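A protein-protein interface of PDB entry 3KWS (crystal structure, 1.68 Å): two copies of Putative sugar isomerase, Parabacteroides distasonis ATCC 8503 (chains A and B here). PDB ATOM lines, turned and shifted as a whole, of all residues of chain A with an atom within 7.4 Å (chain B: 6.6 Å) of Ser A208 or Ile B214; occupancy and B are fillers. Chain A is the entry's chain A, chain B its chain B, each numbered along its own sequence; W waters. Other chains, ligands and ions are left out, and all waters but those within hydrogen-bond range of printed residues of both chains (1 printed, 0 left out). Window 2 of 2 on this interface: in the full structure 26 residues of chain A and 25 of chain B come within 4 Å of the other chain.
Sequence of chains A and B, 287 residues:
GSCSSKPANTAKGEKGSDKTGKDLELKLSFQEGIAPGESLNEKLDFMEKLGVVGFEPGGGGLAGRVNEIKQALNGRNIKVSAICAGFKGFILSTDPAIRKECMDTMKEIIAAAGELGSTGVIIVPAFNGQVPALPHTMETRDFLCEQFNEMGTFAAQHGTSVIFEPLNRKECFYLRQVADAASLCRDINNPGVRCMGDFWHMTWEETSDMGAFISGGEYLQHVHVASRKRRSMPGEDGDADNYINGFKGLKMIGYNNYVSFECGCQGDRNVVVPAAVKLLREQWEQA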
ATOM      1  N   GLN A 177       3.057   0.099   3.458  1.00  0.00           N
ATOM      2  CA  GLN A 177       2.554  -1.127   2.886  1.00  0.00           C
ATOM      3  C   GLN A 177       3.498  -1.810   1.898  1.00  0.00           C
ATOM      4  O   GLN A 177       4.200  -1.150   1.099  1.00  0.00           O
ATOM      5  CB  GLN A 177       1.242  -0.862   2.183  1.00  0.00           C
ATOM      6  CG  GLN A 177       0.172  -0.439   3.186  1.00  0.00           C
ATOM      7  CD  GLN A 177      -1.169  -0.170   2.568  1.00  0.00           C
ATOM      8  OE1 GLN A 177      -1.348   0.814   1.823  1.00  0.00           O
ATOM      9  NE2 GLN A 177      -2.133  -1.043   2.868  1.00  0.00           N
ATOM     10  N   VAL A 178       3.400  -3.130   1.872  1.00  0.00           N
ATOM     11  CA  VAL A 178       4.218  -3.967   0.998  1.00  0.00           C
ATOM     12  C   VAL A 178       3.940  -3.662  -0.471  1.00  0.00           C
ATOM     13  O   VAL A 178       4.883  -3.553  -1.263  1.00  0.00           O
ATOM     14  CB  VAL A 178       4.082  -5.498   1.296  1.00  0.00           C
ATOM     15  CG1 VAL A 178       4.968  -6.292   0.350  1.00  0.00           C
ATOM     16  CG2 VAL A 178       4.470  -5.817   2.786  1.00  0.00           C
ATOM     17  N   MET A 202       2.719  -5.148   9.451  1.00  0.00           N
ATOM     18  CA  MET A 202       1.606  -5.606   8.564  1.00  0.00           C
ATOM     19  C   MET A 202       0.320  -5.770   9.346  1.00  0.00           C
ATOM     20  O   MET A 202      -0.764  -5.577   8.822  1.00  0.00           O
ATOM     21  CB  MET A 202       2.004  -6.901   7.810  1.00  0.00           C
ATOM     22  CG  MET A 202       3.184  -6.735   6.910  1.00  0.00           C
ATOM     23  SD  MET A 202       3.881  -8.434   6.312  1.00  0.00           S
ATOM     24  CE  MET A 202       2.334  -8.974   5.278  1.00  0.00           C
ATOM     25  N   GLU A 205      -1.007  -2.296   9.116  1.00  0.00           N
ATOM     26  CA  GLU A 205      -1.078  -1.604   7.816  1.00  0.00           C
ATOM     27  C   GLU A 205      -1.639  -2.441   6.663  1.00  0.00           C
ATOM     28  O   GLU A 205      -1.964  -1.876   5.623  1.00  0.00           O
ATOM     29  CB  GLU A 205       0.294  -1.056   7.400  1.00  0.00           C
ATOM     30  CG  GLU A 205       0.912  -0.098   8.435  1.00  0.00           C
ATOM     31  CD  GLU A 205       0.050   1.137   8.755  1.00  0.00           C
ATOM     32  OE1 GLU A 205      -0.725   1.587   7.909  1.00  0.00           O
ATOM     33  OE2 GLU A 205       0.189   1.680   9.862  1.00  0.00           O
ATOM     34  N   GLU A 206      -1.754  -3.744   6.857  1.00  0.00           N
ATOM     35  CA  GLU A 206      -2.273  -4.622   5.804  1.00  0.00           C
ATOM     36  C   GLU A 206      -3.596  -5.269   6.169  1.00  0.00           C
ATOM     37  O   GLU A 206      -3.725  -5.923   7.205  1.00  0.00           O
ATOM     38  CB  GLU A 206      -1.307  -5.765   5.495  1.00  0.00           C
ATOM     39  CG  GLU A 206       0.172  -5.347   5.184  1.00  0.00           C
ATOM     40  CD  GLU A 206       0.362  -4.532   3.918  1.00  0.00           C
ATOM     41  OE1 GLU A 206      -0.560  -4.442   3.074  1.00  0.00           O
ATOM     42  OE2 GLU A 206       1.495  -3.970   3.789  1.00  0.00           O
ATOM     43  N   THR A 207      -4.576  -5.124   5.289  1.00  0.00           N
ATOM     44  CA  THR A 207      -5.847  -5.760   5.472  1.00  0.00           C
ATOM     45  C   THR A 207      -5.686  -7.251   5.152  1.00  0.00           C
ATOM     46  O   THR A 207      -6.453  -8.092   5.672  1.00  0.00           O
ATOM     47  CB  THR A 207      -6.940  -5.201   4.535  1.00  0.00           C
ATOM     48  OG1 THR A 207      -6.419  -5.186   3.216  1.00  0.00           O
ATOM     49  CG2 THR A 207      -7.405  -3.820   4.974  1.00  0.00           C
ATOM     50  N   SER A 208      -4.675  -7.592   4.352  1.00  0.00           N
ATOM     51  CA  SER A 208      -4.405  -8.989   3.993  1.00  0.00           C
ATOM     52  C   SER A 208      -2.907  -9.263   3.908  1.00  0.00           C
ATOM     53  O   SER A 208      -2.206  -8.677   3.088  1.00  0.00           O
ATOM     54  CB  SER A 208      -5.037  -9.373   2.644  1.00  0.00           C
ATOM     55  OG  SER A 208      -4.639 -10.688   2.287  1.00  0.00           O
ATOM     56  N   ASP A 209      -2.404 -10.109   4.801  1.00  0.00           N
ATOM     57  CA  ASP A 209      -0.999 -10.501   4.718  1.00  0.00           C
ATOM     58  C   ASP A 209      -0.746 -11.241   3.386  1.00  0.00           C
ATOM     59  O   ASP A 209       0.341 -11.063   2.774  1.00  0.00           O
ATOM     60  CB  ASP A 209      -0.591 -11.415   5.864  1.00  0.00           C
ATOM     61  CG  ASP A 209      -0.644 -10.743   7.234  1.00  0.00           C
ATOM     62  OD1 ASP A 209      -0.592  -9.500   7.333  1.00  0.00           O
ATOM     63  OD2 ASP A 209      -0.818 -11.509   8.197  1.00  0.00           O
ATOM     64  N   MET A 210      -1.687 -12.108   2.992  1.00  0.00           N
ATOM     65  CA  MET A 210      -1.580 -12.836   1.712  1.00  0.00           C
ATOM     66  C   MET A 210      -1.450 -11.866   0.531  1.00  0.00           C
ATOM     67  O   MET A 210      -0.538 -11.981  -0.309  1.00  0.00           O
ATOM     68  CB  MET A 210      -2.739 -13.807   1.524  1.00  0.00           C
ATOM     69  CG  MET A 210      -2.662 -14.570   0.226  1.00  0.00           C
ATOM     70  SD  MET A 210      -4.286 -15.524  -0.228  1.00  0.00           S
ATOM     71  CE  MET A 210      -4.160 -16.631   1.129  1.00  0.00           C
ATOM     72  N   GLY A 211      -2.381 -10.932   0.455  1.00  0.00           N
ATOM     73  CA  GLY A 211      -2.378  -9.946  -0.616  1.00  0.00           C
ATOM     74  C   GLY A 211      -1.120  -9.114  -0.664  1.00  0.00           C
ATOM     75  O   GLY A 211      -0.543  -8.824  -1.716  1.00  0.00           O
ATOM     76  N   ALA A 212      -0.660  -8.746   0.513  1.00  0.00           N
ATOM     77  CA  ALA A 212       0.538  -7.926   0.642  1.00  0.00           C
ATOM     78  C   ALA A 212       1.732  -8.662   0.071  1.00  0.00           C
ATOM     79  O   ALA A 212       2.526  -8.127  -0.727  1.00  0.00           O
ATOM     80  CB  ALA A 212       0.809  -7.610   2.152  1.00  0.00           C
ATOM     81  N   PHE A 213       1.913  -9.900   0.516  1.00  0.00           N
ATOM     82  CA  PHE A 213       3.050 -10.694  -0.001  1.00  0.00           C
ATOM     83  C   PHE A 213       2.936 -11.035  -1.499  1.00  0.00           C
ATOM     84  O   PHE A 213       3.954 -11.060  -2.210  1.00  0.00           O
ATOM     85  CB  PHE A 213       3.228 -11.963   0.810  1.00  0.00           C
ATOM     86  CG  PHE A 213       3.775 -11.773   2.208  1.00  0.00           C
ATOM     87  CD1 PHE A 213       4.762 -10.848   2.515  1.00  0.00           C
ATOM     88  CD2 PHE A 213       3.339 -12.620   3.216  1.00  0.00           C
ATOM     89  CE1 PHE A 213       5.251 -10.744   3.809  1.00  0.00           C
ATOM     90  CE2 PHE A 213       3.859 -12.554   4.496  1.00  0.00           C
ATOM     91  CZ  PHE A 213       4.799 -11.618   4.800  1.00  0.00           C
ATOM     92  N   ILE A 214       1.719 -11.287  -1.993  1.00  0.00           N
ATOM     93  CA  ILE A 214       1.508 -11.505  -3.439  1.00  0.00           C
ATOM     94  C   ILE A 214       1.943 -10.235  -4.211  1.00  0.00           C
ATOM     95  O   ILE A 214       2.654 -10.345  -5.218  1.00  0.00           O
ATOM     96  CB  ILE A 214       0.078 -11.983  -3.752  1.00  0.00           C
ATOM     97  CG1 ILE A 214      -0.107 -13.415  -3.217  1.00  0.00           C
ATOM     98  CG2 ILE A 214      -0.199 -11.969  -5.274  1.00  0.00           C
ATOM     99  CD1 ILE A 214      -1.559 -13.855  -3.255  1.00  0.00           C
ATOM    100  N   ARG A 228       1.810 -10.543  17.524  1.00  0.00           N
ATOM    101  CA  ARG A 228       1.010  -9.506  16.884  1.00  0.00           C
ATOM    102  C   ARG A 228       0.222  -8.515  17.762  1.00  0.00           C
ATOM    103  O   ARG A 228      -0.550  -7.708  17.226  1.00  0.00           O
ATOM    104  CB  ARG A 228       0.099 -10.149  15.796  1.00  0.00           C
ATOM    105  CG  ARG A 228       0.828 -11.130  14.948  1.00  0.00           C
ATOM    106  CD  ARG A 228       0.140 -11.549  13.672  1.00  0.00           C
ATOM    107  NE  ARG A 228       0.234 -10.489  12.668  1.00  0.00           N
ATOM    108  CZ  ARG A 228      -0.038 -10.647  11.368  1.00  0.00           C
ATOM    109  NH1 ARG A 228      -0.438 -11.825  10.894  1.00  0.00           N
ATOM    110  NH2 ARG A 228       0.110  -9.628  10.532  1.00  0.00           N
ATOM    111  N   ASN A 245      -2.350 -16.988   6.761  1.00  0.00           N
ATOM    112  CA  ASN A 245      -2.716 -16.208   5.582  1.00  0.00           C
ATOM    113  C   ASN A 245      -1.450 -15.688   4.891  1.00  0.00           C
ATOM    114  O   ASN A 245      -1.272 -15.822   3.658  1.00  0.00           O
ATOM    115  CB  ASN A 245      -3.690 -15.074   5.989  1.00  0.00           C
ATOM    116  CG  ASN A 245      -4.207 -14.256   4.798  1.00  0.00           C
ATOM    117  OD1 ASN A 245      -3.833 -13.067   4.610  1.00  0.00           O
ATOM    118  ND2 ASN A 245      -5.076 -14.873   3.989  1.00  0.00           N
ATOM    119  N   GLY A 246      -0.549 -15.095   5.667  1.00  0.00           N
ATOM    120  CA  GLY A 246       0.709 -14.615   5.116  1.00  0.00           C
ATOM    121  C   GLY A 246       1.541 -15.753   4.529  1.00  0.00           C
ATOM    122  O   GLY A 246       2.115 -15.650   3.428  1.00  0.00           O
ATOM    123  N   MET A 252       2.551 -19.015  -2.374  1.00  0.00           N
ATOM    124  CA  MET A 252       2.035 -18.699  -3.709  1.00  0.00           C
ATOM    125  C   MET A 252       3.068 -17.990  -4.580  1.00  0.00           C
ATOM    126  O   MET A 252       3.061 -18.180  -5.799  1.00  0.00           O
ATOM    127  CB  MET A 252       0.738 -17.932  -3.587  1.00  0.00           C
ATOM    128  CG  MET A 252      -0.340 -18.754  -2.897  1.00  0.00           C
ATOM    129  SD  MET A 252      -1.795 -17.682  -2.311  1.00  0.00           S
ATOM    130  CE  MET A 252      -2.343 -17.290  -4.127  1.00  0.00           C
ATOM    131  N   VAL B 178      -4.988  -0.148  -4.333  1.00  0.00           N
ATOM    132  CA  VAL B 178      -6.160  -0.753  -3.736  1.00  0.00           C
ATOM    133  C   VAL B 178      -5.875  -1.093  -2.276  1.00  0.00           C
ATOM    134  O   VAL B 178      -6.740  -0.876  -1.418  1.00  0.00           O
ATOM    135  CB  VAL B 178      -6.591  -2.018  -4.507  1.00  0.00           C
ATOM    136  CG1 VAL B 178      -7.790  -2.710  -3.806  1.00  0.00           C
ATOM    137  CG2 VAL B 178      -6.899  -1.681  -5.971  1.00  0.00           C
ATOM    138  N   ARG B 186     -10.746  -0.254   6.303  1.00  0.00           N
ATOM    139  CA  ARG B 186     -10.658  -1.040   7.584  1.00  0.00           C
ATOM    140  C   ARG B 186     -10.596  -0.104   8.796  1.00  0.00           C
ATOM    141  O   ARG B 186     -11.276  -0.325   9.833  1.00  0.00           O
ATOM    142  CB  ARG B 186      -9.452  -1.995   7.583  1.00  0.00           C
ATOM    143  CG  ARG B 186      -9.456  -2.866   8.796  1.00  0.00           C
ATOM    144  CD  ARG B 186      -8.357  -3.935   8.769  1.00  0.00           C
ATOM    145  NE  ARG B 186      -7.010  -3.370   8.827  1.00  0.00           N
ATOM    146  CZ  ARG B 186      -5.922  -4.079   9.138  1.00  0.00           C
ATOM    147  NH1 ARG B 186      -5.989  -5.399   9.338  1.00  0.00           N
ATOM    148  NH2 ARG B 186      -4.752  -3.471   9.197  1.00  0.00           N
ATOM    149  N   ASP B 209      -2.394  -7.543  -9.722  1.00  0.00           N
ATOM    150  CA  ASP B 209      -3.832  -7.312  -9.644  1.00  0.00           C
ATOM    151  C   ASP B 209      -4.470  -8.274  -8.621  1.00  0.00           C
ATOM    152  O   ASP B 209      -5.382  -7.893  -7.862  1.00  0.00           O
ATOM    153  CB  ASP B 209      -4.502  -7.577 -10.984  1.00  0.00           C
ATOM    154  CG  ASP B 209      -4.101  -6.585 -12.074  1.00  0.00           C
ATOM    155  OD1 ASP B 209      -3.694  -5.427 -11.797  1.00  0.00           O
ATOM    156  OD2 ASP B 209      -4.204  -7.002 -13.247  1.00  0.00           O
ATOM    157  N   MET B 210      -4.000  -9.512  -8.601  1.00  0.00           N
ATOM    158  CA  MET B 210      -4.488 -10.477  -7.628  1.00  0.00           C
ATOM    159  C   MET B 210      -4.258 -10.017  -6.187  1.00  0.00           C
ATOM    160  O   MET B 210      -5.198 -10.040  -5.377  1.00  0.00           O
ATOM    161  CB  MET B 210      -3.816 -11.860  -7.822  1.00  0.00           C
ATOM    162  CG  MET B 210      -4.348 -12.890  -6.893  1.00  0.00           C
ATOM    163  SD  MET B 210      -3.279 -14.552  -7.145  1.00  0.00           S
ATOM    164  CE  MET B 210      -3.748 -14.937  -8.762  1.00  0.00           C
ATOM    165  N   GLY B 211      -3.015  -9.636  -5.841  1.00  0.00           N
ATOM    166  CA  GLY B 211      -2.713  -9.206  -4.474  1.00  0.00           C
ATOM    167  C   GLY B 211      -3.510  -7.952  -4.103  1.00  0.00           C
ATOM    168  O   GLY B 211      -3.990  -7.828  -2.981  1.00  0.00           O
ATOM    169  N   ALA B 212      -3.657  -7.033  -5.057  1.00  0.00           N
ATOM    170  CA  ALA B 212      -4.435  -5.816  -4.823  1.00  0.00           C
ATOM    171  C   ALA B 212      -5.878  -6.137  -4.479  1.00  0.00           C
ATOM    172  O   ALA B 212      -6.421  -5.626  -3.479  1.00  0.00           O
ATOM    173  CB  ALA B 212      -4.423  -4.890  -6.050  1.00  0.00           C
ATOM    174  N   PHE B 213      -6.501  -6.998  -5.273  1.00  0.00           N
ATOM    175  CA  PHE B 213      -7.900  -7.347  -5.013  1.00  0.00           C
ATOM    176  C   PHE B 213      -8.045  -8.129  -3.721  1.00  0.00           C
ATOM    177  O   PHE B 213      -9.046  -7.945  -3.004  1.00  0.00           O
ATOM    178  CB  PHE B 213      -8.549  -8.094  -6.191  1.00  0.00           C
ATOM    179  CG  PHE B 213      -8.832  -7.219  -7.422  1.00  0.00           C
ATOM    180  CD1 PHE B 213      -9.353  -5.926  -7.332  1.00  0.00           C
ATOM    181  CD2 PHE B 213      -8.722  -7.792  -8.665  1.00  0.00           C
ATOM    182  CE1 PHE B 213      -9.669  -5.203  -8.453  1.00  0.00           C
ATOM    183  CE2 PHE B 213      -9.086  -7.049  -9.804  1.00  0.00           C
ATOM    184  CZ  PHE B 213      -9.509  -5.776  -9.686  1.00  0.00           C
ATOM    185  N   ILE B 214      -7.091  -9.006  -3.406  1.00  0.00           N
ATOM    186  CA  ILE B 214      -7.097  -9.747  -2.127  1.00  0.00           C
ATOM    187  C   ILE B 214      -7.044  -8.764  -0.946  1.00  0.00           C
ATOM    188  O   ILE B 214      -7.811  -8.924   0.030  1.00  0.00           O
ATOM    189  CB  ILE B 214      -5.988 -10.846  -2.056  1.00  0.00           C
ATOM    190  CG1 ILE B 214      -6.313 -11.928  -3.091  1.00  0.00           C
ATOM    191  CG2 ILE B 214      -5.941 -11.433  -0.664  1.00  0.00           C
ATOM    192  CD1 ILE B 214      -5.204 -13.010  -3.308  1.00  0.00           C
ATOM    193  N   SER B 215      -6.166  -7.753  -1.019  1.00  0.00           N
ATOM    194  CA  SER B 215      -6.128  -6.706   0.005  1.00  0.00           C
ATOM    195  C   SER B 215      -7.477  -5.987   0.059  1.00  0.00           C
ATOM    196  O   SER B 215      -7.983  -5.677   1.119  1.00  0.00           O
ATOM    197  CB  SER B 215      -4.981  -5.736  -0.296  1.00  0.00           C
ATOM    198  OG  SER B 215      -3.748  -6.401  -0.093  1.00  0.00           O
ATOM    199  N   GLY B 216      -8.061  -5.724  -1.117  1.00  0.00           N
ATOM    200  CA  GLY B 216      -9.417  -5.165  -1.169  1.00  0.00           C
ATOM    201  C   GLY B 216     -10.409  -5.965  -0.316  1.00  0.00           C
ATOM    202  O   GLY B 216     -11.117  -5.424   0.525  1.00  0.00           O
ATOM    203  N   GLY B 217     -10.476  -7.260  -0.589  1.00  0.00           N
ATOM    204  CA  GLY B 217     -11.247  -8.195   0.179  1.00  0.00           C
ATOM    205  C   GLY B 217     -12.658  -7.775   0.407  1.00  0.00           C
ATOM    206  O   GLY B 217     -13.348  -7.365  -0.527  1.00  0.00           O
ATOM    207  N   GLU B 218     -13.080  -7.824   1.664  1.00  0.00           N
ATOM    208  CA  GLU B 218     -14.475  -7.516   1.986  1.00  0.00           C
ATOM    209  C   GLU B 218     -14.845  -6.061   1.711  1.00  0.00           C
ATOM    210  O   GLU B 218     -16.020  -5.748   1.642  1.00  0.00           O
ATOM    211  CB  GLU B 218     -14.790  -7.860   3.455  1.00  0.00           C
ATOM    212  CG  GLU B 218     -14.108  -6.895   4.441  1.00  0.00           C
ATOM    213  CD  GLU B 218     -14.172  -7.312   5.875  1.00  0.00           C
ATOM    214  OE1 GLU B 218     -15.203  -7.048   6.507  1.00  0.00           O
ATOM    215  OE2 GLU B 218     -13.121  -7.805   6.369  1.00  0.00           O
ATOM    216  N   LEU B 220     -14.001  -4.447  -1.111  1.00  0.00           N
ATOM    217  CA  LEU B 220     -14.059  -4.217  -2.552  1.00  0.00           C
ATOM    218  C   LEU B 220     -15.484  -4.240  -3.038  1.00  0.00           C
ATOM    219  O   LEU B 220     -16.138  -5.277  -3.006  1.00  0.00           O
ATOM    220  CB  LEU B 220     -13.196  -5.217  -3.291  1.00  0.00           C
ATOM    221  CG  LEU B 220     -12.818  -4.820  -4.733  1.00  0.00           C
ATOM    222  CD1 LEU B 220     -11.612  -3.851  -4.693  1.00  0.00           C
ATOM    223  CD2 LEU B 220     -12.466  -6.012  -5.567  1.00  0.00           C
ATOM    224  N   LYS B 248      -8.432 -14.032 -10.712  1.00  0.00           N
ATOM    225  CA  LYS B 248      -8.147 -15.021  -9.670  1.00  0.00           C
ATOM    226  C   LYS B 248      -8.306 -14.375  -8.288  1.00  0.00           C
ATOM    227  O   LYS B 248      -8.752 -15.047  -7.328  1.00  0.00           O
ATOM    228  CB  LYS B 248      -6.739 -15.561  -9.783  1.00  0.00           C
ATOM    229  CG  LYS B 248      -6.517 -16.574 -10.884  1.00  0.00           C
ATOM    230  CD  LYS B 248      -5.029 -17.032 -11.039  1.00  0.00           C
ATOM    231  CE  LYS B 248      -4.909 -18.050 -12.204  1.00  0.00           C
ATOM    232  NZ  LYS B 248      -5.703 -19.316 -12.013  1.00  0.00           N
ATOM    233  N   GLY B 249      -7.886 -13.126  -8.150  1.00  0.00           N
ATOM    234  CA  GLY B 249      -8.080 -12.391  -6.879  1.00  0.00           C
ATOM    235  C   GLY B 249      -9.551 -12.207  -6.553  1.00  0.00           C
ATOM    236  O   GLY B 249      -9.982 -12.477  -5.444  1.00  0.00           O
ATOM    237  N   LEU B 250     -10.349 -11.839  -7.559  1.00  0.00           N
ATOM    238  CA  LEU B 250     -11.770 -11.644  -7.330  1.00  0.00           C
ATOM    239  C   LEU B 250     -12.432 -12.950  -6.898  1.00  0.00           C
ATOM    240  O   LEU B 250     -13.302 -12.971  -6.015  1.00  0.00           O
ATOM    241  CB  LEU B 250     -12.452 -11.117  -8.578  1.00  0.00           C
ATOM    242  CG  LEU B 250     -12.047  -9.709  -8.985  1.00  0.00           C
ATOM    243  CD1 LEU B 250     -12.869  -9.270 -10.239  1.00  0.00           C
ATOM    244  CD2 LEU B 250     -12.228  -8.694  -7.874  1.00  0.00           C
ATOM    245  N   MET B 252     -10.914 -15.415  -5.312  1.00  0.00           N
ATOM    246  CA  MET B 252     -10.423 -15.816  -4.001  1.00  0.00           C
ATOM    247  C   MET B 252     -11.141 -15.060  -2.878  1.00  0.00           C
ATOM    248  O   MET B 252     -11.333 -15.639  -1.821  1.00  0.00           O
ATOM    249  CB  MET B 252      -8.909 -15.688  -3.943  1.00  0.00           C
ATOM    250  CG  MET B 252      -8.281 -16.640  -4.931  1.00  0.00           C
ATOM    251  SD  MET B 252      -6.442 -16.171  -5.275  1.00  0.00           S
ATOM    252  CE  MET B 252      -5.891 -16.554  -3.439  1.00  0.00           C
ATOM    253  N   ILE B 253     -11.582 -13.824  -3.139  1.00  0.00           N
ATOM    254  CA  ILE B 253     -12.354 -13.046  -2.177  1.00  0.00           C
ATOM    255  C   ILE B 253     -13.887 -13.252  -2.273  1.00  0.00           C
ATOM    256  O   ILE B 253     -14.621 -12.643  -1.469  1.00  0.00           O
ATOM    257  CB  ILE B 253     -12.048 -11.526  -2.212  1.00  0.00           C
ATOM    258  CG1 ILE B 253     -12.588 -10.852  -3.484  1.00  0.00           C
ATOM    259  CG2 ILE B 253     -10.506 -11.258  -2.055  1.00  0.00           C
ATOM    260  CD1 ILE B 253     -12.335  -9.351  -3.500  1.00  0.00           C
HETATM  261  O   HOH W   1      -3.048  -5.602   2.421  1.00  0.00           O
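The backbone carbonyl oxygen (O) of Glu A206 lies within hydrogen-bond range of the guanidinium group (NH1) of Arg B186 (3.2 Å).
The side-chain hydroxyl (OG1) of Thr A207 is in hydrogen-bond range of the backbone carbonyl oxygen (O) of Ser B215, at 2.7 Å.
The backbone NH (N) of Met A210 sits close to the side-chain hydroxyl (OG) of Ser A208 (3.4 Å).
OG of Ser B215 sits at hydrogen-bond distance from O of Gly B211 (3.2 Å).
OD1 of Asn A245 is in hydrogen-bond range of N of Met A210, 2.9 Å away.
OG of Ser A208 sits at hydrogen-bond distance from OD1 of Asn A245, 3.4 Å away.
OE2 of Glu A206 sits at hydrogen-bond distance from N of Val A178, at 2.8 Å.
The side-chain hydroxyl (OG) of Ser A208 is in hydrogen-bond range of the backbone NH (N) of Gly A211.
Among the printed residues, pairs that only touch across the chains: Ser A208 with Ile B214, Gly A211 with Gly B211, Met A252 with Met B252, Ile A214 with Gly B211, Met A210 with Met B252, Ile A214 with Ile B214, Gly A211 with Ile B214, Thr A207 with Arg B186, Gly A211 with Ser B215, Ser A208 with Ser B215, Ala A212 with Ser B215 and Glu A205 with Arg B186.
Gln A177 touches none of the printed residues of chain B.
Printed residues of chain B within 4 Å of Glu A206: Arg B186 (3.2 Å).
Ser A208 touches just these residues of chain B: Ile B214 and Ser B215.
Printed residues of chain B within 4 Å of Ile A214: Gly B211 (3.7 Å) and Ile B214 (3.7 Å).
Ile B214 touches just these residues of chain A: Ser A208 (3.3 Å), Gly A211 (3.8 Å) and Ile A214 (3.7 Å).
Gly B216 touches none of the printed residues of chain A.
The nearest residue of chain A that does not touch Ile B214 is Met A210 (4.1 Å).
Of the 17 printed residues of chain A, 9 touch a printed residue of chain B.
Printed residues of chain A that touch a printed residue of chain B: Glu A205, Glu A206, Thr A207, Ser A208, Met A210, Gly A211, Ala A212, Ile A214 and Met A252.
Hydrophobic or aromatic side chains of chain B that line the printed part of chain A: Ile B214 and Met B252.
Along chain B the printed residues that touch a printed residue of chain A span positions 186 to 252.
Among the printed residues, 14 pairs touch across the chains.
Met A210 touches Met B252, but with the chains exchanged Met A252 does not touch Met B210 (4.2 Å).
Gly A211 touches its own counterpart, Gly B211.
Gly A211 touches Ile B214, and with the chains exchanged Ile A214 touches Gly B211.
Ile B214 touches its own counterpart, Ile A214.
Positions printed for both chains: 178, 209, 210, 211, 212, 213, 214 and 252.
Water W1 lies within hydrogen-bond range of OG of Ser B215, OE1 of Glu A206, N of Ser A208 and N of Thr A207.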
